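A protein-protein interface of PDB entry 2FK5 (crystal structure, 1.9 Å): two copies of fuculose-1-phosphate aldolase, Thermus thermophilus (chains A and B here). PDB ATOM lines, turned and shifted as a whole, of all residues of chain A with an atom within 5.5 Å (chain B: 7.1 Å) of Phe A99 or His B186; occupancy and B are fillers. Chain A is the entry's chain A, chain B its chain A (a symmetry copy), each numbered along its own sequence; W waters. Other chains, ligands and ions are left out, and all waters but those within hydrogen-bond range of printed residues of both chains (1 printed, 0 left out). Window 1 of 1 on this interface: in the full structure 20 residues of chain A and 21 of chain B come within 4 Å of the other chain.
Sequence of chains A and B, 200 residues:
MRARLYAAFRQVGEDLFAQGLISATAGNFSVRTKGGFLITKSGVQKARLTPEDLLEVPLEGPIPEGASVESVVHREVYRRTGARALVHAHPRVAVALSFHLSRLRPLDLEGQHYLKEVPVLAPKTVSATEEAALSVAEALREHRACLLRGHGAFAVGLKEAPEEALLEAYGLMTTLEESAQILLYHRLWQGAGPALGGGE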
ATOM      1  N   ALA A  94     -20.142  -1.766  12.743  1.00  0.00           N
ATOM      2  CA  ALA A  94     -19.912  -1.781  14.190  1.00  0.00           C
ATOM      3  C   ALA A  94     -19.523  -3.186  14.644  1.00  0.00           C
ATOM      4  O   ALA A  94     -18.648  -3.352  15.496  1.00  0.00           O
ATOM      5  CB  ALA A  94     -21.176  -1.307  14.938  1.00  0.00           C
ATOM      6  N   VAL A  95     -20.164  -4.203  14.074  1.00  0.00           N
ATOM      7  CA  VAL A  95     -19.849  -5.575  14.449  1.00  0.00           C
ATOM      8  C   VAL A  95     -18.449  -5.944  13.995  1.00  0.00           C
ATOM      9  O   VAL A  95     -17.721  -6.617  14.719  1.00  0.00           O
ATOM     10  CB  VAL A  95     -20.875  -6.580  13.881  1.00  0.00           C
ATOM     11  CG1 VAL A  95     -20.360  -8.003  14.041  1.00  0.00           C
ATOM     12  CG2 VAL A  95     -22.213  -6.434  14.630  1.00  0.00           C
ATOM     13  N   ALA A  96     -18.059  -5.488  12.806  1.00  0.00           N
ATOM     14  CA  ALA A  96     -16.716  -5.775  12.314  1.00  0.00           C
ATOM     15  C   ALA A  96     -15.712  -5.117  13.253  1.00  0.00           C
ATOM     16  O   ALA A  96     -14.704  -5.721  13.621  1.00  0.00           O
ATOM     17  CB  ALA A  96     -16.541  -5.240  10.893  1.00  0.00           C
ATOM     18  N   LEU A  97     -15.986  -3.881  13.656  1.00  0.00           N
ATOM     19  CA  LEU A  97     -15.069  -3.192  14.563  1.00  0.00           C
ATOM     20  C   LEU A  97     -15.058  -3.820  15.957  1.00  0.00           C
ATOM     21  O   LEU A  97     -14.071  -3.714  16.684  1.00  0.00           O
ATOM     22  CB  LEU A  97     -15.433  -1.709  14.691  1.00  0.00           C
ATOM     23  CG  LEU A  97     -15.535  -0.883  13.407  1.00  0.00           C
ATOM     24  CD1 LEU A  97     -15.343   0.589  13.744  1.00  0.00           C
ATOM     25  CD2 LEU A  97     -14.505  -1.340  12.398  1.00  0.00           C
ATOM     26  N   SER A  98     -16.155  -4.472  16.332  1.00  0.00           N
ATOM     27  CA  SER A  98     -16.237  -5.086  17.654  1.00  0.00           C
ATOM     28  C   SER A  98     -15.153  -6.141  17.890  1.00  0.00           C
ATOM     29  O   SER A  98     -14.780  -6.399  19.038  1.00  0.00           O
ATOM     30  CB  SER A  98     -17.621  -5.705  17.873  1.00  0.00           C
ATOM     31  OG  SER A  98     -17.748  -6.968  17.232  1.00  0.00           O
ATOM     32  N   PHE A  99     -14.646  -6.761  16.828  1.00  0.00           N
ATOM     33  CA  PHE A  99     -13.594  -7.766  17.006  1.00  0.00           C
ATOM     34  C   PHE A  99     -12.272  -7.091  17.328  1.00  0.00           C
ATOM     35  O   PHE A  99     -11.385  -7.708  17.913  1.00  0.00           O
ATOM     36  CB  PHE A  99     -13.381  -8.616  15.742  1.00  0.00           C
ATOM     37  CG  PHE A  99     -14.581  -9.407  15.321  1.00  0.00           C
ATOM     38  CD1 PHE A  99     -15.462  -8.896  14.377  1.00  0.00           C
ATOM     39  CD2 PHE A  99     -14.837 -10.659  15.872  1.00  0.00           C
ATOM     40  CE1 PHE A  99     -16.585  -9.621  13.986  1.00  0.00           C
ATOM     41  CE2 PHE A  99     -15.958 -11.392  15.487  1.00  0.00           C
ATOM     42  CZ  PHE A  99     -16.832 -10.871  14.543  1.00  0.00           C
ATOM     43  N   HIS A 100     -12.158  -5.818  16.953  1.00  0.00           N
ATOM     44  CA  HIS A 100     -10.928  -5.050  17.130  1.00  0.00           C
ATOM     45  C   HIS A 100     -10.881  -4.037  18.261  1.00  0.00           C
ATOM     46  O   HIS A 100      -9.827  -3.459  18.517  1.00  0.00           O
ATOM     47  CB  HIS A 100     -10.600  -4.310  15.831  1.00  0.00           C
ATOM     48  CG  HIS A 100     -10.261  -5.214  14.689  1.00  0.00           C
ATOM     49  ND1 HIS A 100     -10.842  -5.091  13.444  1.00  0.00           N
ATOM     50  CD2 HIS A 100      -9.387  -6.245  14.596  1.00  0.00           C
ATOM     51  CE1 HIS A 100     -10.340  -6.006  12.633  1.00  0.00           C
ATOM     52  NE2 HIS A 100      -9.454  -6.719  13.308  1.00  0.00           N
ATOM     53  N   LEU A 101     -12.005  -3.807  18.935  1.00  0.00           N
ATOM     54  CA  LEU A 101     -12.029  -2.812  20.008  1.00  0.00           C
ATOM     55  C   LEU A 101     -12.640  -3.358  21.295  1.00  0.00           C
ATOM     56  O   LEU A 101     -13.433  -4.296  21.265  1.00  0.00           O
ATOM     57  CB  LEU A 101     -12.848  -1.595  19.561  1.00  0.00           C
ATOM     58  CG  LEU A 101     -12.519  -0.917  18.225  1.00  0.00           C
ATOM     59  CD1 LEU A 101     -13.686  -0.028  17.818  1.00  0.00           C
ATOM     60  CD2 LEU A 101     -11.233  -0.109  18.341  1.00  0.00           C
ATOM     61  N   ARG A 149     -19.518  -8.656  20.965  1.00  0.00           N
ATOM     62  CA  ARG A 149     -18.535  -9.042  19.965  1.00  0.00           C
ATOM     63  C   ARG A 149     -19.007 -10.123  19.014  1.00  0.00           C
ATOM     64  O   ARG A 149     -19.418 -11.204  19.427  1.00  0.00           O
ATOM     65  CB  ARG A 149     -17.224  -9.467  20.631  1.00  0.00           C
ATOM     66  CG  ARG A 149     -16.152  -9.902  19.632  1.00  0.00           C
ATOM     67  CD  ARG A 149     -14.781  -9.899  20.271  1.00  0.00           C
ATOM     68  NE  ARG A 149     -14.377  -8.547  20.641  1.00  0.00           N
ATOM     69  CZ  ARG A 149     -13.408  -8.262  21.504  1.00  0.00           C
ATOM     70  NH1 ARG A 149     -12.740  -9.247  22.093  1.00  0.00           N
ATOM     71  N   GLY A 150     -18.970  -9.799  17.727  1.00  0.00           N
ATOM     72  CA  GLY A 150     -19.360 -10.750  16.705  1.00  0.00           C
ATOM     73  C   GLY A 150     -20.832 -11.066  16.591  1.00  0.00           C
ATOM     74  O   GLY A 150     -21.215 -11.915  15.786  1.00  0.00           O
ATOM     75  N   PRO B 106     -17.537 -17.389   8.037  1.00  0.00           N
ATOM     76  CA  PRO B 106     -18.001 -16.206   8.768  1.00  0.00           C
ATOM     77  C   PRO B 106     -17.344 -15.993  10.122  1.00  0.00           C
ATOM     78  O   PRO B 106     -17.015 -16.946  10.818  1.00  0.00           O
ATOM     79  CB  PRO B 106     -19.498 -16.456   8.920  1.00  0.00           C
ATOM     80  CG  PRO B 106     -19.834 -17.316   7.735  1.00  0.00           C
ATOM     81  CD  PRO B 106     -18.666 -18.272   7.706  1.00  0.00           C
ATOM     82  N   LEU B 107     -17.175 -14.730  10.492  1.00  0.00           N
ATOM     83  CA  LEU B 107     -16.607 -14.363  11.786  1.00  0.00           C
ATOM     84  C   LEU B 107     -17.740 -14.092  12.773  1.00  0.00           C
ATOM     85  O   LEU B 107     -17.568 -14.225  13.985  1.00  0.00           O
ATOM     86  CB  LEU B 107     -15.775 -13.086  11.663  1.00  0.00           C
ATOM     87  CG  LEU B 107     -14.460 -13.117  10.885  1.00  0.00           C
ATOM     88  CD1 LEU B 107     -13.934 -11.701  10.757  1.00  0.00           C
ATOM     89  CD2 LEU B 107     -13.448 -13.998  11.608  1.00  0.00           C
ATOM     90  N   ASP B 108     -18.898 -13.701  12.243  1.00  0.00           N
ATOM     91  CA  ASP B 108     -20.049 -13.364  13.084  1.00  0.00           C
ATOM     92  C   ASP B 108     -20.897 -14.563  13.475  1.00  0.00           C
ATOM     93  O   ASP B 108     -20.998 -15.527  12.728  1.00  0.00           O
ATOM     94  CB  ASP B 108     -20.927 -12.333  12.377  1.00  0.00           C
ATOM     95  CG  ASP B 108     -21.481 -12.848  11.059  1.00  0.00           C
ATOM     96  OD1 ASP B 108     -20.681 -13.132  10.144  1.00  0.00           O
ATOM     97  OD2 ASP B 108     -22.716 -12.969  10.942  1.00  0.00           O
ATOM     98  N   LEU B 109     -21.522 -14.484  14.647  1.00  0.00           N
ATOM     99  CA  LEU B 109     -22.344 -15.585  15.143  1.00  0.00           C
ATOM    100  C   LEU B 109     -23.451 -16.029  14.198  1.00  0.00           C
ATOM    101  O   LEU B 109     -23.624 -17.225  13.969  1.00  0.00           O
ATOM    102  CB  LEU B 109     -22.962 -15.228  16.494  1.00  0.00           C
ATOM    103  CG  LEU B 109     -23.686 -16.389  17.188  1.00  0.00           C
ATOM    104  CD2 LEU B 109     -24.370 -15.877  18.451  1.00  0.00           C
ATOM    105  N   GLN B 112     -21.903 -17.960  11.393  1.00  0.00           N
ATOM    106  CA  GLN B 112     -21.360 -19.246  11.810  1.00  0.00           C
ATOM    107  C   GLN B 112     -22.480 -20.238  12.090  1.00  0.00           C
ATOM    108  O   GLN B 112     -22.353 -21.424  11.797  1.00  0.00           O
ATOM    109  CB  GLN B 112     -20.485 -19.090  13.052  1.00  0.00           C
ATOM    110  CG  GLN B 112     -19.322 -18.144  12.852  1.00  0.00           C
ATOM    111  CD  GLN B 112     -18.400 -18.096  14.039  1.00  0.00           C
ATOM    112  OE1 GLN B 112     -18.830 -18.272  15.180  1.00  0.00           O
ATOM    113  NE2 GLN B 112     -17.121 -17.836  13.785  1.00  0.00           N
ATOM    114  N   ALA B 180     -19.929 -11.677   4.532  1.00  0.00           N
ATOM    115  CA  ALA B 180     -18.844 -11.308   3.611  1.00  0.00           C
ATOM    116  C   ALA B 180     -18.408  -9.859   3.860  1.00  0.00           C
ATOM    117  O   ALA B 180     -17.213  -9.553   3.890  1.00  0.00           O
ATOM    118  CB  ALA B 180     -19.305 -11.473   2.168  1.00  0.00           C
ATOM    119  N   GLN B 181     -19.380  -8.970   4.029  1.00  0.00           N
ATOM    120  CA  GLN B 181     -19.076  -7.566   4.306  1.00  0.00           C
ATOM    121  C   GLN B 181     -18.338  -7.448   5.636  1.00  0.00           C
ATOM    122  O   GLN B 181     -17.363  -6.720   5.738  1.00  0.00           O
ATOM    123  CB  GLN B 181     -20.366  -6.735   4.334  1.00  0.00           C
ATOM    124  CG  GLN B 181     -21.066  -6.723   2.968  1.00  0.00           C
ATOM    125  CD  GLN B 181     -22.273  -5.812   2.919  1.00  0.00           C
ATOM    126  OE1 GLN B 181     -22.824  -5.444   3.948  1.00  0.00           O
ATOM    127  NE2 GLN B 181     -22.697  -5.453   1.711  1.00  0.00           N
ATOM    128  N   ILE B 182     -18.805  -8.159   6.657  1.00  0.00           N
ATOM    129  CA  ILE B 182     -18.127  -8.115   7.954  1.00  0.00           C
ATOM    130  C   ILE B 182     -16.676  -8.581   7.802  1.00  0.00           C
ATOM    131  O   ILE B 182     -15.756  -7.987   8.383  1.00  0.00           O
ATOM    132  CB  ILE B 182     -18.878  -8.977   8.999  1.00  0.00           C
ATOM    133  CG1 ILE B 182     -20.184  -8.273   9.385  1.00  0.00           C
ATOM    134  CG2 ILE B 182     -18.010  -9.197  10.245  1.00  0.00           C
ATOM    135  CD1 ILE B 182     -21.066  -9.093  10.330  1.00  0.00           C
ATOM    136  N   LEU B 183     -16.467  -9.636   7.017  1.00  0.00           N
ATOM    137  CA  LEU B 183     -15.111 -10.138   6.769  1.00  0.00           C
ATOM    138  C   LEU B 183     -14.254  -9.053   6.117  1.00  0.00           C
ATOM    139  O   LEU B 183     -13.107  -8.814   6.514  1.00  0.00           O
ATOM    140  CB  LEU B 183     -15.152 -11.363   5.844  1.00  0.00           C
ATOM    141  CG  LEU B 183     -15.458 -12.715   6.488  1.00  0.00           C
ATOM    142  CD1 LEU B 183     -15.712 -13.772   5.415  1.00  0.00           C
ATOM    143  CD2 LEU B 183     -14.271 -13.123   7.357  1.00  0.00           C
ATOM    144  N   LEU B 184     -14.813  -8.401   5.104  1.00  0.00           N
ATOM    145  CA  LEU B 184     -14.094  -7.345   4.397  1.00  0.00           C
ATOM    146  C   LEU B 184     -13.774  -6.177   5.333  1.00  0.00           C
ATOM    147  O   LEU B 184     -12.632  -5.738   5.415  1.00  0.00           O
ATOM    148  CB  LEU B 184     -14.923  -6.827   3.210  1.00  0.00           C
ATOM    149  CG  LEU B 184     -14.380  -5.571   2.497  1.00  0.00           C
ATOM    150  CD1 LEU B 184     -13.055  -5.890   1.791  1.00  0.00           C
ATOM    151  CD2 LEU B 184     -15.408  -5.079   1.480  1.00  0.00           C
ATOM    152  N   TYR B 185     -14.784  -5.671   6.034  1.00  0.00           N
ATOM    153  CA  TYR B 185     -14.577  -4.543   6.943  1.00  0.00           C
ATOM    154  C   TYR B 185     -13.535  -4.891   8.006  1.00  0.00           C
ATOM    155  O   TYR B 185     -12.662  -4.094   8.320  1.00  0.00           O
ATOM    156  CB  TYR B 185     -15.885  -4.172   7.634  1.00  0.00           C
ATOM    157  CG  TYR B 185     -16.993  -3.721   6.700  1.00  0.00           C
ATOM    158  CD1 TYR B 185     -18.326  -3.945   7.032  1.00  0.00           C
ATOM    159  CD2 TYR B 185     -16.713  -3.035   5.521  1.00  0.00           C
ATOM    160  CE1 TYR B 185     -19.358  -3.501   6.222  1.00  0.00           C
ATOM    161  CE2 TYR B 185     -17.744  -2.579   4.693  1.00  0.00           C
ATOM    162  CZ  TYR B 185     -19.065  -2.817   5.056  1.00  0.00           C
ATOM    163  OH  TYR B 185     -20.100  -2.372   4.270  1.00  0.00           O
ATOM    164  N   HIS B 186     -13.654  -6.080   8.574  1.00  0.00           N
ATOM    165  CA  HIS B 186     -12.705  -6.532   9.588  1.00  0.00           C
ATOM    166  C   HIS B 186     -11.268  -6.502   9.034  1.00  0.00           C
ATOM    167  O   HIS B 186     -10.339  -6.025   9.692  1.00  0.00           O
ATOM    168  CB  HIS B 186     -13.097  -7.948  10.025  1.00  0.00           C
ATOM    169  CG  HIS B 186     -12.115  -8.599  10.941  1.00  0.00           C
ATOM    170  ND1 HIS B 186     -10.952  -9.185  10.490  1.00  0.00           N
ATOM    171  CD2 HIS B 186     -12.121  -8.761  12.285  1.00  0.00           C
ATOM    172  CE1 HIS B 186     -10.283  -9.678  11.518  1.00  0.00           C
ATOM    173  NE2 HIS B 186     -10.972  -9.433  12.618  1.00  0.00           N
ATOM    174  N   ARG B 187     -11.098  -6.986   7.811  1.00  0.00           N
ATOM    175  CA  ARG B 187      -9.779  -7.027   7.180  1.00  0.00           C
ATOM    176  C   ARG B 187      -9.231  -5.640   6.817  1.00  0.00           C
ATOM    177  O   ARG B 187      -8.038  -5.371   6.997  1.00  0.00           O
ATOM    178  CB  ARG B 187      -9.851  -7.906   5.930  1.00  0.00           C
ATOM    179  CG  ARG B 187      -8.534  -8.121   5.206  1.00  0.00           C
ATOM    180  CD  ARG B 187      -8.758  -9.209   4.174  1.00  0.00           C
ATOM    181  NE  ARG B 187      -7.682  -9.365   3.209  1.00  0.00           N
ATOM    182  CZ  ARG B 187      -6.861 -10.409   3.168  1.00  0.00           C
ATOM    183  NH1 ARG B 187      -6.982 -11.388   4.051  1.00  0.00           N
ATOM    184  NH2 ARG B 187      -5.943 -10.491   2.219  1.00  0.00           N
ATOM    185  N   LEU B 188     -10.089  -4.764   6.293  1.00  0.00           N
ATOM    186  CA  LEU B 188      -9.650  -3.419   5.920  1.00  0.00           C
ATOM    187  C   LEU B 188      -9.251  -2.596   7.148  1.00  0.00           C
ATOM    188  O   LEU B 188      -8.281  -1.850   7.095  1.00  0.00           O
ATOM    189  CB  LEU B 188     -10.736  -2.672   5.117  1.00  0.00           C
ATOM    190  CG  LEU B 188     -11.199  -3.270   3.780  1.00  0.00           C
ATOM    191  CD1 LEU B 188     -11.965  -2.196   2.982  1.00  0.00           C
ATOM    192  CD2 LEU B 188     -10.000  -3.759   2.962  1.00  0.00           C
ATOM    193  N   TRP B 189     -10.001  -2.725   8.243  1.00  0.00           N
ATOM    194  CA  TRP B 189      -9.677  -2.008   9.480  1.00  0.00           C
ATOM    195  C   TRP B 189      -8.297  -2.460   9.968  1.00  0.00           C
ATOM    196  O   TRP B 189      -7.435  -1.647  10.315  1.00  0.00           O
ATOM    197  CB  TRP B 189     -10.733  -2.303  10.560  1.00  0.00           C
ATOM    198  CG  TRP B 189     -10.427  -1.695  11.894  1.00  0.00           C
ATOM    199  CD1 TRP B 189      -9.647  -2.224  12.887  1.00  0.00           C
ATOM    200  CD2 TRP B 189     -10.880  -0.428  12.372  1.00  0.00           C
ATOM    201  NE1 TRP B 189      -9.588  -1.358  13.955  1.00  0.00           N
ATOM    202  CE2 TRP B 189     -10.335  -0.249  13.665  1.00  0.00           C
ATOM    203  CE3 TRP B 189     -11.691   0.577  11.832  1.00  0.00           C
ATOM    204  CZ2 TRP B 189     -10.582   0.899  14.426  1.00  0.00           C
ATOM    205  CZ3 TRP B 189     -11.932   1.719  12.590  1.00  0.00           C
ATOM    206  CH2 TRP B 189     -11.377   1.867  13.873  1.00  0.00           C
ATOM    207  N   GLN B 190      -8.091  -3.769   9.989  1.00  0.00           N
ATOM    208  CA  GLN B 190      -6.815  -4.334  10.433  1.00  0.00           C
ATOM    209  C   GLN B 190      -5.681  -3.906   9.507  1.00  0.00           C
ATOM    210  O   GLN B 190      -4.581  -3.576   9.959  1.00  0.00           O
ATOM    211  CB  GLN B 190      -6.914  -5.859  10.455  1.00  0.00           C
ATOM    212  CG  GLN B 190      -5.601  -6.598  10.667  1.00  0.00           C
ATOM    213  CD  GLN B 190      -5.116  -6.537  12.100  1.00  0.00           C
ATOM    214  OE1 GLN B 190      -5.803  -6.014  12.978  1.00  0.00           O
ATOM    215  NE2 GLN B 190      -3.928  -7.082  12.348  1.00  0.00           N
ATOM    216  N   GLY B 191      -5.958  -3.912   8.208  1.00  0.00           N
ATOM    217  CA  GLY B 191      -4.951  -3.545   7.229  1.00  0.00           C
ATOM    218  C   GLY B 191      -4.523  -2.091   7.280  1.00  0.00           C
ATOM    219  O   GLY B 191      -3.401  -1.761   6.900  1.00  0.00           O
HETATM  220  O   HOH W   1      -8.185  -1.302  16.476  1.00  0.00           O
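No position is printed for both chains. Of the 12 pairs that touch across the chains among the printed residues, none has its exchanged pair printed and touching as well.
The side-chain hydroxyl (OG) of Ser A98 is in hydrogen-bond range of the backbone carbonyl oxygen (O) of Val A95, 2.5 Å away. OG of Ser A98 lies within hydrogen-bond range of N of Gly A150 (3.1 Å).
NE2 of His A100 sits at hydrogen-bond distance from NE2 of His B186 (3.2 Å). N of Leu B109 lies within hydrogen-bond range of O of Gly A150, 2.8 Å away.
Val A95 touches Ile B182. CB of Ala A96 touches O of Ile B182 (3.8 Å). Ala A96 touches Tyr B185 (CB to CB, 3.5 Å). Ala A96 touches His B186 (CB to N, 3.8 Å). Trp B189 touches Leu A97. CZ of Phe A99 touches O of Leu B107, at 3.5 Å. Phe A99 touches His B186 (CB to CD2, 3.7 Å). His A100 touches Trp B189. NE2 of His A100 touches OE1 of Gln B190 (3.7 Å). Gly A150 touches Asp B108.
Water W1 bridges NE1 of Trp B189 (2.9 Å) and O of His A100 (3.4 Å).
Phe A99 touches just these residues of chain B: Leu B107 and His B186. Printed residues of chain A within 4 Å of His B186: Ala A96 (3.8 Å), Phe A99 (3.7 Å) and His A100 (2.9 Å). Of the printed residues of chain A, Trp B189 touches Leu A97 (3.5 Å) and His A100 (3.2 Å). Of the printed residues of chain A, Gln B190 touches His A100 (3.7 Å). Printed residues of chain A within 4 Å of Tyr B185: Ala A96. Of the printed residues of chain B, Val A95 touches Ile B182. Of the printed residues of chain A, Leu B109 touches Gly A150 (2.8 Å). Leu B183 touches none of the printed residues of chain A. The nearest residue of chain B that does not touch Phe A99 is Ile B182 (4.03 Å). The nearest printed residue of chain A that does not touch Asp B108 is Phe A99 (4.2 Å).
Printed residues of chain B that touch a printed residue of chain A: Leu B107, Asp B108, Leu B109, Ile B182, Tyr B185, His B186, Trp B189 and Gln B190. Hydrophobic or aromatic side chains of chain B that line the printed part of chain A: Leu B107, Leu B109, Ile B182, Tyr B185, His B186 and Trp B189. Hydrophobic or aromatic side chains of chain A that line the printed part of chain B: Val A95, Ala A96, Leu A97, Phe A99 and His A100. Among the printed residues, 12 pairs touch across the chains.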
